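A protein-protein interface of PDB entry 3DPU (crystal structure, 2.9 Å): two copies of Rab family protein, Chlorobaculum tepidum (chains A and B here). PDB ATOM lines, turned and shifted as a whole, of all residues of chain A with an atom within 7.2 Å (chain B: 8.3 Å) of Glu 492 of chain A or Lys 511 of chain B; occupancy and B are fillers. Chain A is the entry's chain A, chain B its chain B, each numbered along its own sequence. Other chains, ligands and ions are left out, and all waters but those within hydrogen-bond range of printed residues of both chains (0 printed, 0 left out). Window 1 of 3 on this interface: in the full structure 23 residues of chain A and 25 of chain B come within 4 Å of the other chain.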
ATOM      1  N   VAL A 477     -23.043  -0.152 -26.862  1.00  0.00           N
ATOM      2  CA  VAL A 477     -22.063  -1.013 -27.497  1.00  0.00           C
ATOM      3  C   VAL A 477     -21.710  -2.192 -26.595  1.00  0.00           C
ATOM      4  O   VAL A 477     -21.400  -2.011 -25.421  1.00  0.00           O
ATOM      5  CB  VAL A 477     -20.783  -0.224 -27.869  1.00  0.00           C
ATOM      6  CG1 VAL A 477     -19.720  -1.155 -28.453  1.00  0.00           C
ATOM      7  CG2 VAL A 477     -21.103   0.894 -28.853  1.00  0.00           C
ATOM      8  N   LYS A 478     -21.782  -3.398 -27.150  1.00  0.00           N
ATOM      9  CA  LYS A 478     -21.285  -4.598 -26.490  1.00  0.00           C
ATOM     10  C   LYS A 478     -20.066  -5.140 -27.235  1.00  0.00           C
ATOM     11  O   LYS A 478     -20.038  -5.214 -28.469  1.00  0.00           O
ATOM     12  CB  LYS A 478     -22.367  -5.673 -26.402  1.00  0.00           C
ATOM     13  CG  LYS A 478     -23.314  -5.501 -25.222  1.00  0.00           C
ATOM     14  CD  LYS A 478     -24.369  -6.613 -25.166  1.00  0.00           C
ATOM     15  CE  LYS A 478     -25.478  -6.389 -26.185  1.00  0.00           C
ATOM     16  NZ  LYS A 478     -26.635  -7.311 -25.958  1.00  0.00           N
ATOM     17  N   GLU A 479     -19.058  -5.527 -26.469  1.00  0.00           N
ATOM     18  CA  GLU A 479     -17.797  -5.973 -27.030  1.00  0.00           C
ATOM     19  C   GLU A 479     -17.650  -7.478 -26.922  1.00  0.00           C
ATOM     20  O   GLU A 479     -17.888  -8.065 -25.871  1.00  0.00           O
ATOM     21  CB  GLU A 479     -16.659  -5.247 -26.332  1.00  0.00           C
ATOM     22  CG  GLU A 479     -16.825  -3.744 -26.451  1.00  0.00           C
ATOM     23  CD  GLU A 479     -16.084  -2.972 -25.399  1.00  0.00           C
ATOM     24  OE1 GLU A 479     -15.767  -3.554 -24.335  1.00  0.00           O
ATOM     25  OE2 GLU A 479     -15.822  -1.775 -25.642  1.00  0.00           O
ATOM     26  N   PHE A 480     -17.270  -8.091 -28.035  1.00  0.00           N
ATOM     27  CA  PHE A 480     -17.162  -9.537 -28.137  1.00  0.00           C
ATOM     28  C   PHE A 480     -15.762  -9.982 -28.547  1.00  0.00           C
ATOM     29  O   PHE A 480     -14.934  -9.174 -28.971  1.00  0.00           O
ATOM     30  CB  PHE A 480     -18.174 -10.064 -29.146  1.00  0.00           C
ATOM     31  CG  PHE A 480     -19.595  -9.988 -28.683  1.00  0.00           C
ATOM     32  CD1 PHE A 480     -20.434  -8.979 -29.144  1.00  0.00           C
ATOM     33  CD2 PHE A 480     -20.107 -10.939 -27.801  1.00  0.00           C
ATOM     34  CE1 PHE A 480     -21.770  -8.910 -28.719  1.00  0.00           C
ATOM     35  CE2 PHE A 480     -21.423 -10.890 -27.373  1.00  0.00           C
ATOM     36  CZ  PHE A 480     -22.266  -9.873 -27.834  1.00  0.00           C
ATOM     37  N   ILE A 481     -15.521 -11.281 -28.414  1.00  0.00           N
ATOM     38  CA  ILE A 481     -14.259 -11.919 -28.762  1.00  0.00           C
ATOM     39  C   ILE A 481     -14.618 -13.287 -29.338  1.00  0.00           C
ATOM     40  O   ILE A 481     -15.300 -14.066 -28.679  1.00  0.00           O
ATOM     41  CB  ILE A 481     -13.385 -12.097 -27.504  1.00  0.00           C
ATOM     42  CG1 ILE A 481     -12.901 -10.741 -27.006  1.00  0.00           C
ATOM     43  CG2 ILE A 481     -12.195 -13.015 -27.761  1.00  0.00           C
ATOM     44  CD1 ILE A 481     -12.853 -10.646 -25.500  1.00  0.00           C
ATOM     45  N   LEU A 490     -19.103 -16.255 -30.553  1.00  0.00           N
ATOM     46  CA  LEU A 490     -18.619 -15.103 -29.806  1.00  0.00           C
ATOM     47  C   LEU A 490     -18.976 -15.144 -28.331  1.00  0.00           C
ATOM     48  O   LEU A 490     -20.062 -15.558 -27.959  1.00  0.00           O
ATOM     49  CB  LEU A 490     -19.139 -13.805 -30.422  1.00  0.00           C
ATOM     50  CG  LEU A 490     -18.830 -13.559 -31.894  1.00  0.00           C
ATOM     51  CD1 LEU A 490     -19.466 -12.258 -32.346  1.00  0.00           C
ATOM     52  CD2 LEU A 490     -17.337 -13.533 -32.127  1.00  0.00           C
ATOM     53  N   VAL A 491     -18.040 -14.700 -27.502  1.00  0.00           N
ATOM     54  CA  VAL A 491     -18.255 -14.545 -26.069  1.00  0.00           C
ATOM     55  C   VAL A 491     -18.143 -13.059 -25.709  1.00  0.00           C
ATOM     56  O   VAL A 491     -17.347 -12.325 -26.285  1.00  0.00           O
ATOM     57  CB  VAL A 491     -17.264 -15.416 -25.238  1.00  0.00           C
ATOM     58  CG1 VAL A 491     -15.826 -15.015 -25.496  1.00  0.00           C
ATOM     59  CG2 VAL A 491     -17.564 -15.321 -23.761  1.00  0.00           C
ATOM     60  N   GLU A 492     -18.960 -12.618 -24.769  1.00  0.00           N
ATOM     61  CA  GLU A 492     -18.971 -11.221 -24.406  1.00  0.00           C
ATOM     62  C   GLU A 492     -17.797 -10.968 -23.484  1.00  0.00           C
ATOM     63  O   GLU A 492     -17.563 -11.716 -22.546  1.00  0.00           O
ATOM     64  CB  GLU A 492     -20.310 -10.832 -23.759  1.00  0.00           C
ATOM     65  CG  GLU A 492     -20.391  -9.369 -23.312  1.00  0.00           C
ATOM     66  CD  GLU A 492     -21.801  -8.776 -23.398  1.00  0.00           C
ATOM     67  OE1 GLU A 492     -21.935  -7.540 -23.222  1.00  0.00           O
ATOM     68  OE2 GLU A 492     -22.773  -9.532 -23.647  1.00  0.00           O
ATOM     69  N   TYR A 493     -17.046  -9.919 -23.768  1.00  0.00           N
ATOM     70  CA  TYR A 493     -15.916  -9.543 -22.950  1.00  0.00           C
ATOM     71  C   TYR A 493     -16.323  -9.301 -21.486  1.00  0.00           C
ATOM     72  O   TYR A 493     -15.611  -9.703 -20.553  1.00  0.00           O
ATOM     73  CB  TYR A 493     -15.262  -8.328 -23.585  1.00  0.00           C
ATOM     74  CG  TYR A 493     -14.150  -7.688 -22.813  1.00  0.00           C
ATOM     75  CD1 TYR A 493     -12.916  -8.322 -22.658  1.00  0.00           C
ATOM     76  CD2 TYR A 493     -14.317  -6.411 -22.277  1.00  0.00           C
ATOM     77  CE1 TYR A 493     -11.877  -7.707 -21.960  1.00  0.00           C
ATOM     78  CE2 TYR A 493     -13.287  -5.779 -21.583  1.00  0.00           C
ATOM     79  CZ  TYR A 493     -12.070  -6.431 -21.423  1.00  0.00           C
ATOM     80  OH  TYR A 493     -11.066  -5.791 -20.736  1.00  0.00           O
ATOM     81  N   LYS A 494     -17.483  -8.673 -21.288  1.00  0.00           N
ATOM     82  CA  LYS A 494     -18.063  -8.512 -19.949  1.00  0.00           C
ATOM     83  C   LYS A 494     -18.255  -9.860 -19.238  1.00  0.00           C
ATOM     84  O   LYS A 494     -18.112  -9.949 -18.022  1.00  0.00           O
ATOM     85  CB  LYS A 494     -19.398  -7.755 -20.019  1.00  0.00           C
ATOM     86  CG  LYS A 494     -19.278  -6.235 -20.180  1.00  0.00           C
ATOM     87  N   GLU A 495     -18.571 -10.901 -20.007  1.00  0.00           N
ATOM     88  CA  GLU A 495     -18.746 -12.250 -19.472  1.00  0.00           C
ATOM     89  C   GLU A 495     -17.473 -12.811 -18.869  1.00  0.00           C
ATOM     90  O   GLU A 495     -17.458 -13.276 -17.730  1.00  0.00           O
ATOM     91  CB  GLU A 495     -19.251 -13.191 -20.556  1.00  0.00           C
ATOM     92  CG  GLU A 495     -20.619 -13.748 -20.260  1.00  0.00           C
ATOM     93  CD  GLU A 495     -20.577 -14.936 -19.311  1.00  0.00           C
ATOM     94  OE1 GLU A 495     -21.581 -15.181 -18.606  1.00  0.00           O
ATOM     95  OE2 GLU A 495     -19.537 -15.631 -19.276  1.00  0.00           O
ATOM     96  N   LEU A 496     -16.406 -12.754 -19.652  1.00  0.00           N
ATOM     97  CA  LEU A 496     -15.103 -13.210 -19.215  1.00  0.00           C
ATOM     98  C   LEU A 496     -14.617 -12.470 -17.966  1.00  0.00           C
ATOM     99  O   LEU A 496     -14.282 -13.117 -16.963  1.00  0.00           O
ATOM    100  CB  LEU A 496     -14.097 -13.110 -20.359  1.00  0.00           C
ATOM    101  CG  LEU A 496     -14.481 -13.909 -21.609  1.00  0.00           C
ATOM    102  CD1 LEU A 496     -13.369 -13.847 -22.645  1.00  0.00           C
ATOM    103  CD2 LEU A 496     -14.775 -15.361 -21.236  1.00  0.00           C
ATOM    104  N   LEU A 497     -14.607 -11.134 -18.001  1.00  0.00           N
ATOM    105  CA  LEU A 497     -14.187 -10.353 -16.821  1.00  0.00           C
ATOM    106  C   LEU A 497     -14.977 -10.786 -15.593  1.00  0.00           C
ATOM    107  O   LEU A 497     -14.405 -11.008 -14.529  1.00  0.00           O
ATOM    108  CB  LEU A 497     -14.330  -8.839 -17.040  1.00  0.00           C
ATOM    109  CG  LEU A 497     -13.541  -8.146 -18.161  1.00  0.00           C
ATOM    110  CD1 LEU A 497     -14.176  -6.793 -18.502  1.00  0.00           C
ATOM    111  CD2 LEU A 497     -12.049  -7.994 -17.834  1.00  0.00           C
ATOM    112  N   GLY A 498     -16.289 -10.926 -15.763  1.00  0.00           N
ATOM    113  CA  GLY A 498     -17.170 -11.420 -14.710  1.00  0.00           C
ATOM    114  C   GLY A 498     -16.809 -12.812 -14.213  1.00  0.00           C
ATOM    115  O   GLY A 498     -17.005 -13.132 -13.032  1.00  0.00           O
ATOM    116  N   LEU A 499     -16.276 -13.638 -15.116  1.00  0.00           N
ATOM    117  CA  LEU A 499     -15.865 -14.984 -14.767  1.00  0.00           C
ATOM    118  C   LEU A 499     -14.563 -14.930 -13.986  1.00  0.00           C
ATOM    119  O   LEU A 499     -14.309 -15.777 -13.124  1.00  0.00           O
ATOM    120  CB  LEU A 499     -15.742 -15.860 -16.019  1.00  0.00           C
ATOM    121  CG  LEU A 499     -17.034 -16.361 -16.696  1.00  0.00           C
ATOM    122  CD1 LEU A 499     -16.765 -17.097 -18.004  1.00  0.00           C
ATOM    123  CD2 LEU A 499     -17.845 -17.241 -15.760  1.00  0.00           C
ATOM    124  N   MET A 502     -15.436 -13.726 -10.392  1.00  0.00           N
ATOM    125  CA  MET A 502     -15.975 -14.901  -9.702  1.00  0.00           C
ATOM    126  C   MET A 502     -14.870 -15.829  -9.246  1.00  0.00           C
ATOM    127  O   MET A 502     -15.076 -16.657  -8.358  1.00  0.00           O
ATOM    128  CB  MET A 502     -16.923 -15.680 -10.611  1.00  0.00           C
ATOM    129  CG  MET A 502     -18.220 -14.967 -10.908  1.00  0.00           C
ATOM    130  SD  MET A 502     -19.252 -15.874 -12.072  1.00  0.00           S
ATOM    131  CE  MET A 502     -20.116 -16.988 -10.964  1.00  0.00           C
ATOM    132  N   TYR A 507     -14.408 -21.114 -19.317  1.00  0.00           N
ATOM    133  CA  TYR A 507     -15.558 -20.712 -20.096  1.00  0.00           C
ATOM    134  C   TYR A 507     -16.075 -21.930 -20.823  1.00  0.00           C
ATOM    135  O   TYR A 507     -15.412 -22.472 -21.700  1.00  0.00           O
ATOM    136  CB  TYR A 507     -15.241 -19.608 -21.092  1.00  0.00           C
ATOM    137  CG  TYR A 507     -16.459 -19.274 -21.933  1.00  0.00           C
ATOM    138  CD1 TYR A 507     -17.499 -18.490 -21.411  1.00  0.00           C
ATOM    139  CD2 TYR A 507     -16.598 -19.775 -23.231  1.00  0.00           C
ATOM    140  CE1 TYR A 507     -18.617 -18.198 -22.159  1.00  0.00           C
ATOM    141  CE2 TYR A 507     -17.714 -19.480 -23.987  1.00  0.00           C
ATOM    142  CZ  TYR A 507     -18.720 -18.692 -23.443  1.00  0.00           C
ATOM    143  OH  TYR A 507     -19.839 -18.401 -24.192  1.00  0.00           O
ATOM    144  N   LEU A 522      -8.395 -13.862 -22.538  1.00  0.00           N
ATOM    145  CA  LEU A 522      -8.527 -12.525 -21.980  1.00  0.00           C
ATOM    146  C   LEU A 522      -7.206 -11.752 -22.075  1.00  0.00           C
ATOM    147  O   LEU A 522      -7.191 -10.558 -22.375  1.00  0.00           O
ATOM    148  CB  LEU A 522      -9.010 -12.625 -20.534  1.00  0.00           C
ATOM    149  CG  LEU A 522     -10.022 -11.590 -20.055  1.00  0.00           C
ATOM    150  CD1 LEU A 522     -11.024 -11.233 -21.149  1.00  0.00           C
ATOM    151  CD2 LEU A 522     -10.731 -12.096 -18.808  1.00  0.00           C
ATOM    152  N   LEU B 483     -32.866 -16.601 -18.189  1.00  0.00           N
ATOM    153  CA  LEU B 483     -32.428 -16.803 -16.821  1.00  0.00           C
ATOM    154  C   LEU B 483     -33.537 -16.466 -15.805  1.00  0.00           C
ATOM    155  O   LEU B 483     -34.122 -15.386 -15.875  1.00  0.00           O
ATOM    156  CB  LEU B 483     -31.186 -15.936 -16.587  1.00  0.00           C
ATOM    157  CG  LEU B 483     -29.787 -16.548 -16.771  1.00  0.00           C
ATOM    158  CD1 LEU B 483     -29.795 -17.900 -17.471  1.00  0.00           C
ATOM    159  CD2 LEU B 483     -28.856 -15.590 -17.488  1.00  0.00           C
ATOM    160  N   ASP B 488     -34.183 -10.310 -19.460  1.00  0.00           N
ATOM    161  CA  ASP B 488     -33.356  -9.678 -20.500  1.00  0.00           C
ATOM    162  C   ASP B 488     -32.220 -10.589 -20.972  1.00  0.00           C
ATOM    163  O   ASP B 488     -31.683 -10.426 -22.065  1.00  0.00           O
ATOM    164  CB  ASP B 488     -32.786  -8.347 -19.995  1.00  0.00           C
ATOM    165  N   GLU B 489     -31.872 -11.559 -20.138  1.00  0.00           N
ATOM    166  CA  GLU B 489     -30.703 -12.373 -20.362  1.00  0.00           C
ATOM    167  C   GLU B 489     -31.093 -13.770 -20.870  1.00  0.00           C
ATOM    168  O   GLU B 489     -31.502 -14.646 -20.102  1.00  0.00           O
ATOM    169  CB  GLU B 489     -29.879 -12.431 -19.069  1.00  0.00           C
ATOM    170  CG  GLU B 489     -28.382 -12.309 -19.285  1.00  0.00           C
ATOM    171  CD  GLU B 489     -27.971 -10.930 -19.771  1.00  0.00           C
ATOM    172  OE1 GLU B 489     -28.696  -9.954 -19.464  1.00  0.00           O
ATOM    173  OE2 GLU B 489     -26.921 -10.816 -20.454  1.00  0.00           O
ATOM    174  N   TYR B 507     -25.162 -23.603 -14.747  1.00  0.00           N
ATOM    175  CA  TYR B 507     -24.877 -22.664 -15.818  1.00  0.00           C
ATOM    176  C   TYR B 507     -24.289 -21.431 -15.175  1.00  0.00           C
ATOM    177  O   TYR B 507     -24.895 -20.852 -14.270  1.00  0.00           O
ATOM    178  CB  TYR B 507     -26.122 -22.287 -16.605  1.00  0.00           C
ATOM    179  CG  TYR B 507     -25.840 -21.209 -17.607  1.00  0.00           C
ATOM    180  CD1 TYR B 507     -25.188 -21.501 -18.792  1.00  0.00           C
ATOM    181  CD2 TYR B 507     -26.194 -19.887 -17.357  1.00  0.00           C
ATOM    182  CE1 TYR B 507     -24.905 -20.515 -19.714  1.00  0.00           C
ATOM    183  CE2 TYR B 507     -25.908 -18.876 -18.277  1.00  0.00           C
ATOM    184  CZ  TYR B 507     -25.263 -19.204 -19.452  1.00  0.00           C
ATOM    185  OH  TYR B 507     -24.976 -18.239 -20.375  1.00  0.00           O
ATOM    186  N   VAL B 508     -23.112 -21.026 -15.639  1.00  0.00           N
ATOM    187  CA  VAL B 508     -22.400 -19.934 -14.990  1.00  0.00           C
ATOM    188  C   VAL B 508     -22.434 -18.620 -15.787  1.00  0.00           C
ATOM    189  O   VAL B 508     -21.971 -18.545 -16.926  1.00  0.00           O
ATOM    190  CB  VAL B 508     -20.972 -20.373 -14.558  1.00  0.00           C
ATOM    191  CG1 VAL B 508     -20.233 -21.018 -15.715  1.00  0.00           C
ATOM    192  CG2 VAL B 508     -20.195 -19.208 -13.994  1.00  0.00           C
ATOM    193  N   SER B 509     -23.008 -17.597 -15.158  1.00  0.00           N
ATOM    194  CA  SER B 509     -23.164 -16.276 -15.763  1.00  0.00           C
ATOM    195  C   SER B 509     -22.112 -15.340 -15.218  1.00  0.00           C
ATOM    196  O   SER B 509     -22.057 -15.109 -14.012  1.00  0.00           O
ATOM    197  CB  SER B 509     -24.552 -15.698 -15.470  1.00  0.00           C
ATOM    198  OG  SER B 509     -24.683 -14.398 -16.023  1.00  0.00           O
ATOM    199  N   GLY B 510     -21.284 -14.808 -16.111  1.00  0.00           N
ATOM    200  CA  GLY B 510     -20.227 -13.865 -15.747  1.00  0.00           C
ATOM    201  C   GLY B 510     -20.730 -12.442 -15.619  1.00  0.00           C
ATOM    202  O   GLY B 510     -20.369 -11.747 -14.671  1.00  0.00           O
ATOM    203  N   LYS B 511     -21.570 -12.018 -16.571  1.00  0.00           N
ATOM    204  CA  LYS B 511     -22.142 -10.659 -16.595  1.00  0.00           C
ATOM    205  C   LYS B 511     -22.733 -10.280 -15.250  1.00  0.00           C
ATOM    206  O   LYS B 511     -22.519  -9.175 -14.758  1.00  0.00           O
ATOM    207  CB  LYS B 511     -23.219 -10.516 -17.683  1.00  0.00           C
ATOM    208  CG  LYS B 511     -22.720  -9.981 -19.028  1.00  0.00           C
ATOM    209  CD  LYS B 511     -23.881  -9.603 -19.954  1.00  0.00           C
ATOM    210  N   LEU B 512     -23.492 -11.206 -14.673  1.00  0.00           N
ATOM    211  CA  LEU B 512     -23.996 -11.083 -13.312  1.00  0.00           C
ATOM    212  C   LEU B 512     -23.446 -12.269 -12.562  1.00  0.00           C
ATOM    213  O   LEU B 512     -23.738 -13.408 -12.917  1.00  0.00           O
ATOM    214  CB  LEU B 512     -25.526 -11.068 -13.294  1.00  0.00           C
ATOM    215  CG  LEU B 512     -26.248 -11.747 -14.452  1.00  0.00           C
ATOM    216  CD1 LEU B 512     -26.846 -13.053 -13.999  1.00  0.00           C
ATOM    217  CD2 LEU B 512     -27.323 -10.820 -14.971  1.00  0.00           C
ATOM    218  N   GLU B 513     -22.629 -12.003 -11.550  1.00  0.00           N
ATOM    219  CA  GLU B 513     -21.814 -13.034 -10.903  1.00  0.00           C
ATOM    220  C   GLU B 513     -22.660 -14.094 -10.187  1.00  0.00           C
ATOM    221  O   GLU B 513     -22.685 -14.151  -8.956  1.00  0.00           O
ATOM    222  CB  GLU B 513     -20.820 -12.373  -9.941  1.00  0.00           C
ATOM    223  N   LYS B 514     -23.337 -14.930 -10.979  1.00  0.00           N
ATOM    224  CA  LYS B 514     -24.361 -15.869 -10.500  1.00  0.00           C
ATOM    225  C   LYS B 514     -24.293 -17.196 -11.246  1.00  0.00           C
ATOM    226  O   LYS B 514     -23.954 -17.235 -12.434  1.00  0.00           O
ATOM    227  CB  LYS B 514     -25.769 -15.281 -10.672  1.00  0.00           C
ATOM    228  CG  LYS B 514     -26.189 -14.295  -9.590  1.00  0.00           C
ATOM    229  CD  LYS B 514     -27.702 -14.306  -9.379  1.00  0.00           C
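OE1 of Glu 495 of chain A lies within hydrogen-bond range of N of Gly 510 of chain B.
The side-chain sulfur (SD) of Met 502 of chain A lies close to the backbone carbonyl oxygen (O) of Ser 509 of chain B (3.5 Å).
O of Lys 514 of chain B is in hydrogen-bond range of N of Ser 509 of chain B.
The side-chain hydroxyl (OG) of Ser 509 of chain B lies close to the backbone carbonyl oxygen (O) of Leu 512 of chain B, at 3.4 Å.
Of the 11 printed residues of chain B, 6 touch a printed residue of chain A.
Hydrophobic or aromatic side chains of chain A that line the printed part of chain B: Leu 499 and Met 502.
Among the printed residues, no Asp or Glu carboxylate lies within 4 Å of a Lys or Arg side-chain nitrogen of the other chain.
Among the printed residues, merely in contact across the chains: Gly 498 of chain A with Gly 510 of chain B, Glu 495 of chain A with Ser 509 of chain B, Leu 499 of chain A with Val 508 of chain B, Met 502 of chain A with Val 508 of chain B, Glu 495 of chain A with Lys 511 of chain B, Glu 495 of chain A with Val 508 of chain B, Met 502 of chain A with Glu 513 of chain B, Met 502 of chain A with Lys 514 of chain B and Glu 492 of chain A with Lys 511 of chain B.
Position printed for both chains: 507.
Of the 11 pairs that touch across the chains among the printed residues, none has its exchanged pair printed and touching as well.
Phe 480 of chain A touches none of the printed residues of chain B.
No residue of chain B comes within 4 Å of Val 491 of chain A.
Printed residues of chain B within 4 Å of Glu 492 of chain A: Lys 511 (3.9 Å).
Tyr 493 of chain A touches none of the printed residues of chain B.
Of the printed residues of chain B, Gly 498 of chain A touches Gly 510 (3.2 Å).
Printed residues of chain B within 4 Å of Leu 499 of chain A: Val 508 (3.5 Å).
Printed residues of chain A within 4 Å of Val 508 of chain B: Glu 495 (3.8 Å), Leu 499 (3.5 Å) and Met 502 (3.8 Å).
Of the printed residues of chain A, Gly 510 of chain B touches Glu 495 (2.5 Å) and Gly 498 (3.2 Å).
Lys 511 of chain B touches just these residues of chain A: Glu 492 (3.9 Å) and Glu 495 (3.8 Å).
Of the printed residues of chain A, Lys 514 of chain B touches Met 502 (3.8 Å).
The nearest residue of chain A that does not touch Lys 511 of chain B is Lys 494 of chain A (4.1 Å).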
